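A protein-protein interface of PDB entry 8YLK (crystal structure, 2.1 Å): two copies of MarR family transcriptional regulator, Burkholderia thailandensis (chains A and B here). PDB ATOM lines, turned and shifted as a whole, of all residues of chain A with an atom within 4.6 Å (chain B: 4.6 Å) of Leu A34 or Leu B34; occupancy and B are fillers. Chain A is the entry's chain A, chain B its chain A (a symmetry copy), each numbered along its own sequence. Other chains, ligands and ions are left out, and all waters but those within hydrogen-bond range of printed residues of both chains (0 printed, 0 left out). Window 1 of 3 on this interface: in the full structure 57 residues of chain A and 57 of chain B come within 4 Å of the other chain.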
ATOM      1  N   VAL A  30     -17.422  27.144  27.416  1.00  0.00           N
ATOM      2  CA  VAL A  30     -17.863  26.813  26.063  1.00  0.00           C
ATOM      3  C   VAL A  30     -19.380  26.640  26.011  1.00  0.00           C
ATOM      4  O   VAL A  30     -20.042  27.139  25.092  1.00  0.00           O
ATOM      5  CB  VAL A  30     -17.112  25.568  25.548  1.00  0.00           C
ATOM      6  CG1 VAL A  30     -17.150  24.442  26.574  1.00  0.00           C
ATOM      7  CG2 VAL A  30     -17.677  25.108  24.208  1.00  0.00           C
ATOM      8  N   LEU A  31     -19.962  25.960  27.001  1.00  0.00           N
ATOM      9  CA  LEU A  31     -21.407  25.750  26.988  1.00  0.00           C
ATOM     10  C   LEU A  31     -22.173  27.003  27.401  1.00  0.00           C
ATOM     11  O   LEU A  31     -23.305  27.211  26.948  1.00  0.00           O
ATOM     12  CB  LEU A  31     -21.785  24.574  27.898  1.00  0.00           C
ATOM     13  CG  LEU A  31     -21.336  23.176  27.460  1.00  0.00           C
ATOM     14  CD1 LEU A  31     -21.693  22.142  28.518  1.00  0.00           C
ATOM     15  CD2 LEU A  31     -21.954  22.793  26.123  1.00  0.00           C
ATOM     16  N   GLY A  32     -21.595  27.834  28.268  1.00  0.00           N
ATOM     17  CA  GLY A  32     -22.224  29.108  28.574  1.00  0.00           C
ATOM     18  C   GLY A  32     -22.196  30.051  27.388  1.00  0.00           C
ATOM     19  O   GLY A  32     -23.178  30.747  27.112  1.00  0.00           O
ATOM     20  N   ARG A  33     -21.080  30.075  26.656  1.00  0.00           N
ATOM     21  CA  ARG A  33     -21.017  30.895  25.452  1.00  0.00           C
ATOM     22  C   ARG A  33     -21.881  30.326  24.336  1.00  0.00           C
ATOM     23  O   ARG A  33     -22.419  31.087  23.523  1.00  0.00           O
ATOM     24  CB  ARG A  33     -19.569  31.044  24.990  1.00  0.00           C
ATOM     25  CG  ARG A  33     -18.761  31.963  25.879  1.00  0.00           C
ATOM     26  CD  ARG A  33     -17.397  32.255  25.290  1.00  0.00           C
ATOM     27  NE  ARG A  33     -16.619  33.085  26.199  1.00  0.00           N
ATOM     28  CZ  ARG A  33     -15.294  33.107  26.242  1.00  0.00           C
ATOM     29  NH1 ARG A  33     -14.586  32.343  25.424  1.00  0.00           N
ATOM     30  NH2 ARG A  33     -14.679  33.893  27.112  1.00  0.00           N
ATOM     31  N   LEU A  34     -22.030  29.002  24.277  1.00  0.00           N
ATOM     32  CA  LEU A  34     -22.925  28.405  23.293  1.00  0.00           C
ATOM     33  C   LEU A  34     -24.362  28.855  23.525  1.00  0.00           C
ATOM     34  O   LEU A  34     -25.061  29.263  22.589  1.00  0.00           O
ATOM     35  CB  LEU A  34     -22.823  26.879  23.353  1.00  0.00           C
ATOM     36  CG  LEU A  34     -23.777  26.078  22.463  1.00  0.00           C
ATOM     37  CD1 LEU A  34     -23.300  26.105  21.026  1.00  0.00           C
ATOM     38  CD2 LEU A  34     -23.889  24.646  22.948  1.00  0.00           C
ATOM     39  N   GLN A  35     -24.821  28.791  24.777  1.00  0.00           N
ATOM     40  CA  GLN A  35     -26.210  29.131  25.061  1.00  0.00           C
ATOM     41  C   GLN A  35     -26.449  30.629  24.932  1.00  0.00           C
ATOM     42  O   GLN A  35     -27.484  31.055  24.406  1.00  0.00           O
ATOM     43  CB  GLN A  35     -26.596  28.637  26.455  1.00  0.00           C
ATOM     44  CG  GLN A  35     -26.549  27.119  26.601  1.00  0.00           C
ATOM     45  CD  GLN A  35     -27.057  26.642  27.951  1.00  0.00           C
ATOM     46  OE1 GLN A  35     -28.244  26.370  28.119  1.00  0.00           O
ATOM     47  NE2 GLN A  35     -26.155  26.539  28.920  1.00  0.00           N
ATOM     48  N   GLU A  36     -25.508  31.446  25.407  1.00  0.00           N
ATOM     49  CA  GLU A  36     -25.692  32.891  25.325  1.00  0.00           C
ATOM     50  C   GLU A  36     -25.671  33.372  23.879  1.00  0.00           C
ATOM     51  O   GLU A  36     -26.451  34.255  23.502  1.00  0.00           O
ATOM     52  CB  GLU A  36     -24.624  33.604  26.153  1.00  0.00           C
ATOM     53  CG  GLU A  36     -24.723  35.128  26.132  1.00  0.00           C
ATOM     54  CD  GLU A  36     -25.913  35.664  26.912  1.00  0.00           C
ATOM     55  OE1 GLU A  36     -26.752  34.864  27.383  1.00  0.00           O
ATOM     56  OE2 GLU A  36     -26.003  36.899  27.058  1.00  0.00           O
ATOM     57  N   ALA A  37     -24.788  32.807  23.054  1.00  0.00           N
ATOM     58  CA  ALA A  37     -24.744  33.201  21.650  1.00  0.00           C
ATOM     59  C   ALA A  37     -26.026  32.807  20.932  1.00  0.00           C
ATOM     60  O   ALA A  37     -26.579  33.599  20.159  1.00  0.00           O
ATOM     61  CB  ALA A  37     -23.531  32.582  20.962  1.00  0.00           C
ATOM     62  N   ALA A  38     -26.526  31.594  21.184  1.00  0.00           N
ATOM     63  CA  ALA A  38     -27.783  31.186  20.567  1.00  0.00           C
ATOM     64  C   ALA A  38     -28.934  32.076  21.019  1.00  0.00           C
ATOM     65  O   ALA A  38     -29.815  32.417  20.221  1.00  0.00           O
ATOM     66  CB  ALA A  38     -28.082  29.725  20.895  1.00  0.00           C
ATOM     67  N   ILE A  41     -28.378  35.899  19.538  1.00  0.00           N
ATOM     68  CA  ILE A  41     -28.586  35.955  18.096  1.00  0.00           C
ATOM     69  C   ILE A  41     -30.060  35.760  17.757  1.00  0.00           C
ATOM     70  O   ILE A  41     -30.631  36.513  16.960  1.00  0.00           O
ATOM     71  CB  ILE A  41     -27.692  34.926  17.384  1.00  0.00           C
ATOM     72  CG1 ILE A  41     -26.227  35.352  17.482  1.00  0.00           C
ATOM     73  CG2 ILE A  41     -28.103  34.771  15.929  1.00  0.00           C
ATOM     74  CD1 ILE A  41     -25.261  34.321  16.936  1.00  0.00           C
ATOM     75  N   LEU A 158     -19.335  22.486  15.908  1.00  0.00           N
ATOM     76  CA  LEU A 158     -20.723  22.338  16.338  1.00  0.00           C
ATOM     77  C   LEU A 158     -21.314  21.012  15.879  1.00  0.00           C
ATOM     78  O   LEU A 158     -22.136  20.421  16.590  1.00  0.00           O
ATOM     79  CB  LEU A 158     -21.568  23.503  15.821  1.00  0.00           C
ATOM     80  CG  LEU A 158     -21.340  24.855  16.499  1.00  0.00           C
ATOM     81  CD1 LEU A 158     -22.109  25.941  15.778  1.00  0.00           C
ATOM     82  CD2 LEU A 158     -21.743  24.797  17.970  1.00  0.00           C
ATOM     83  N   LEU A 161     -19.897  18.364  18.270  1.00  0.00           N
ATOM     84  CA  LEU A 161     -20.600  18.467  19.543  1.00  0.00           C
ATOM     85  C   LEU A 161     -22.025  17.939  19.428  1.00  0.00           C
ATOM     86  O   LEU A 161     -22.524  17.265  20.339  1.00  0.00           O
ATOM     87  CB  LEU A 161     -20.602  19.922  20.017  1.00  0.00           C
ATOM     88  CG  LEU A 161     -21.256  20.225  21.363  1.00  0.00           C
ATOM     89  CD1 LEU A 161     -20.563  19.457  22.483  1.00  0.00           C
ATOM     90  CD2 LEU A 161     -21.222  21.719  21.634  1.00  0.00           C
ATOM     91  N   VAL B  30     -23.885  27.064  10.008  1.00  0.00           N
ATOM     92  CA  VAL B  30     -23.263  27.371  11.293  1.00  0.00           C
ATOM     93  C   VAL B  30     -24.301  27.881  12.292  1.00  0.00           C
ATOM     94  O   VAL B  30     -24.309  27.471  13.459  1.00  0.00           O
ATOM     95  CB  VAL B  30     -22.098  28.363  11.098  1.00  0.00           C
ATOM     96  CG1 VAL B  30     -22.526  29.551  10.245  1.00  0.00           C
ATOM     97  CG2 VAL B  30     -21.547  28.825  12.444  1.00  0.00           C
ATOM     98  N   LEU B  31     -25.206  28.758  11.854  1.00  0.00           N
ATOM     99  CA  LEU B  31     -26.207  29.291  12.772  1.00  0.00           C
ATOM    100  C   LEU B  31     -27.320  28.286  13.056  1.00  0.00           C
ATOM    101  O   LEU B  31     -27.905  28.305  14.146  1.00  0.00           O
ATOM    102  CB  LEU B  31     -26.799  30.595  12.222  1.00  0.00           C
ATOM    103  CG  LEU B  31     -25.870  31.811  12.148  1.00  0.00           C
ATOM    104  CD1 LEU B  31     -26.574  32.985  11.484  1.00  0.00           C
ATOM    105  CD2 LEU B  31     -25.376  32.210  13.532  1.00  0.00           C
ATOM    106  N   GLY B  32     -27.644  27.421  12.094  1.00  0.00           N
ATOM    107  CA  GLY B  32     -28.591  26.356  12.374  1.00  0.00           C
ATOM    108  C   GLY B  32     -28.026  25.334  13.340  1.00  0.00           C
ATOM    109  O   GLY B  32     -28.726  24.860  14.239  1.00  0.00           O
ATOM    110  N   ARG B  33     -26.745  24.993  13.183  1.00  0.00           N
ATOM    111  CA  ARG B  33     -26.113  24.082  14.129  1.00  0.00           C
ATOM    112  C   ARG B  33     -25.899  24.737  15.487  1.00  0.00           C
ATOM    113  O   ARG B  33     -25.945  24.053  16.515  1.00  0.00           O
ATOM    114  CB  ARG B  33     -24.791  23.567  13.565  1.00  0.00           C
ATOM    115  CG  ARG B  33     -24.980  22.566  12.446  1.00  0.00           C
ATOM    116  CD  ARG B  33     -23.671  21.922  12.044  1.00  0.00           C
ATOM    117  NE  ARG B  33     -23.875  21.015  10.923  1.00  0.00           N
ATOM    118  CZ  ARG B  33     -22.937  20.694  10.041  1.00  0.00           C
ATOM    119  NH1 ARG B  33     -21.719  21.204  10.146  1.00  0.00           N
ATOM    120  NH2 ARG B  33     -23.225  19.866   9.050  1.00  0.00           N
ATOM    121  N   LEU B  34     -25.667  26.050  15.514  1.00  0.00           N
ATOM    122  CA  LEU B  34     -25.555  26.751  16.789  1.00  0.00           C
ATOM    123  C   LEU B  34     -26.858  26.662  17.572  1.00  0.00           C
ATOM    124  O   LEU B  34     -26.862  26.346  18.769  1.00  0.00           O
ATOM    125  CB  LEU B  34     -25.169  28.212  16.547  1.00  0.00           C
ATOM    126  CG  LEU B  34     -25.112  29.131  17.770  1.00  0.00           C
ATOM    127  CD1 LEU B  34     -23.847  28.874  18.562  1.00  0.00           C
ATOM    128  CD2 LEU B  34     -25.179  30.587  17.352  1.00  0.00           C
ATOM    129  N   GLN B  35     -27.982  26.935  16.908  1.00  0.00           N
ATOM    130  CA  GLN B  35     -29.260  26.947  17.611  1.00  0.00           C
ATOM    131  C   GLN B  35     -29.695  25.538  17.990  1.00  0.00           C
ATOM    132  O   GLN B  35     -30.212  25.317  19.091  1.00  0.00           O
ATOM    133  CB  GLN B  35     -30.325  27.633  16.755  1.00  0.00           C
ATOM    134  CG  GLN B  35     -30.037  29.107  16.485  1.00  0.00           C
ATOM    135  CD  GLN B  35     -31.164  29.800  15.741  1.00  0.00           C
ATOM    136  OE1 GLN B  35     -32.080  30.349  16.352  1.00  0.00           O
ATOM    137  NE2 GLN B  35     -31.103  29.775  14.415  1.00  0.00           N
ATOM    138  N   GLU B  36     -29.497  24.571  17.093  1.00  0.00           N
ATOM    139  CA  GLU B  36     -29.910  23.205  17.397  1.00  0.00           C
ATOM    140  C   GLU B  36     -29.076  22.610  18.525  1.00  0.00           C
ATOM    141  O   GLU B  36     -29.607  21.901  19.387  1.00  0.00           O
ATOM    142  CB  GLU B  36     -29.824  22.339  16.140  1.00  0.00           C
ATOM    143  CG  GLU B  36     -30.230  20.882  16.349  1.00  0.00           C
ATOM    144  CD  GLU B  36     -31.725  20.700  16.564  1.00  0.00           C
ATOM    145  OE1 GLU B  36     -32.459  21.708  16.675  1.00  0.00           O
ATOM    146  OE2 GLU B  36     -32.167  19.535  16.615  1.00  0.00           O
ATOM    147  N   ALA B  37     -27.771  22.886  18.539  1.00  0.00           N
ATOM    148  CA  ALA B  37     -26.928  22.376  19.614  1.00  0.00           C
ATOM    149  C   ALA B  37     -27.317  22.990  20.952  1.00  0.00           C
ATOM    150  O   ALA B  37     -27.406  22.283  21.962  1.00  0.00           O
ATOM    151  CB  ALA B  37     -25.457  22.641  19.308  1.00  0.00           C
ATOM    152  N   ALA B  38     -27.565  24.303  20.977  1.00  0.00           N
ATOM    153  CA  ALA B  38     -27.996  24.933  22.219  1.00  0.00           C
ATOM    154  C   ALA B  38     -29.332  24.372  22.690  1.00  0.00           C
ATOM    155  O   ALA B  38     -29.543  24.175  23.892  1.00  0.00           O
ATOM    156  CB  ALA B  38     -28.092  26.446  22.038  1.00  0.00           C
ATOM    157  N   ILE B  41     -28.850  20.411  23.785  1.00  0.00           N
ATOM    158  CA  ILE B  41     -28.088  20.282  25.022  1.00  0.00           C
ATOM    159  C   ILE B  41     -28.905  20.780  26.210  1.00  0.00           C
ATOM    160  O   ILE B  41     -28.984  20.112  27.248  1.00  0.00           O
ATOM    161  CB  ILE B  41     -26.742  21.015  24.904  1.00  0.00           C
ATOM    162  CG1 ILE B  41     -25.830  20.275  23.926  1.00  0.00           C
ATOM    163  CG2 ILE B  41     -26.074  21.136  26.263  1.00  0.00           C
ATOM    164  CD1 ILE B  41     -24.536  21.008  23.633  1.00  0.00           C
ATOM    165  N   LEU B 158     -16.833  31.043  19.611  1.00  0.00           N
ATOM    166  CA  LEU B 158     -18.091  31.540  20.161  1.00  0.00           C
ATOM    167  C   LEU B 158     -17.927  32.923  20.778  1.00  0.00           C
ATOM    168  O   LEU B 158     -18.848  33.744  20.713  1.00  0.00           O
ATOM    169  CB  LEU B 158     -18.643  30.561  21.197  1.00  0.00           C
ATOM    170  CG  LEU B 158     -19.222  29.254  20.647  1.00  0.00           C
ATOM    171  CD1 LEU B 158     -19.570  28.316  21.784  1.00  0.00           C
ATOM    172  CD2 LEU B 158     -20.447  29.528  19.781  1.00  0.00           C
ATOM    173  N   LEU B 161     -17.817  35.370  17.822  1.00  0.00           N
ATOM    174  CA  LEU B 161     -19.173  35.538  17.312  1.00  0.00           C
ATOM    175  C   LEU B 161     -20.021  36.367  18.269  1.00  0.00           C
ATOM    176  O   LEU B 161     -20.817  37.211  17.838  1.00  0.00           O
ATOM    177  CB  LEU B 161     -19.811  34.168  17.075  1.00  0.00           C
ATOM    178  CG  LEU B 161     -21.223  34.138  16.495  1.00  0.00           C
ATOM    179  CD1 LEU B 161     -21.259  34.819  15.132  1.00  0.00           C
ATOM    180  CD2 LEU B 161     -21.714  32.705  16.393  1.00  0.00           C
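Among the printed residues, merely in contact across the chains: Ala A38 with Ala B38 (3.5 Å), Val A30 with Leu B158 (3.5 Å), Leu A158 with Val B30 (3.5 Å), Leu A34 with Leu B158 (3.6 Å), Leu A158 with Leu B34 (3.6 Å), Leu A34 with Leu B34 (3.7 Å), Ile A41 with Leu B34 (3.8 Å), Leu A34 with Ile B41 (3.8 Å), Arg A33 with Leu B158 (3.9 Å), Leu A158 with Arg B33 (3.9 Å), Leu A161 with Ile B41 (3.9 Å) and Ile A41 with Leu B161 (3.9 Å).
Arg A33 touches Leu B158, and with the chains exchanged Leu A158 touches Arg B33.
Leu A34 touches Ile B41, and with the chains exchanged Ile A41 touches Leu B34.
Leu A34 touches Leu B158, and with the chains exchanged Leu A158 touches Leu B34.
Ala B38 touches its own counterpart, Ala A38.
Of the 12 printed residues of chain A, 7 touch a printed residue of chain B.
Hydrophobic or aromatic side chains of chain A that line the printed part of chain B: Leu A34, Ala A38, Ile A41, Leu A158 and Leu A161.
Printed residues of chain B that touch a printed residue of chain A: Val B30, Arg B33, Leu B34, Ala B38, Ile B41, Leu B158 and Leu B161.
Hydrophobic or aromatic side chains of chain B that line the printed part of chain A: Leu B34, Ala B38, Ile B41, Leu B158 and Leu B161.
Leu A34 touches just these residues of chain B: Leu B34, Ile B41 and Leu B158.
Of chain A, only Leu A34 (3.7 Å), Ile A41 (3.8 Å) and Leu A158 (3.6 Å) come within 4 Å of Leu B34.
Printed residues of chain A within 4 Å of Leu B158: Val A30 (3.5 Å), Arg A33 (3.9 Å) and Leu A34 (3.6 Å).
Of the printed residues of chain B, Ala A38 touches Ala B38 (3.5 Å).
Glu A36 touches none of the printed residues of chain B.
The nearest residue of chain B that does not touch Leu A34 is Ala B38 (4.2 Å).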
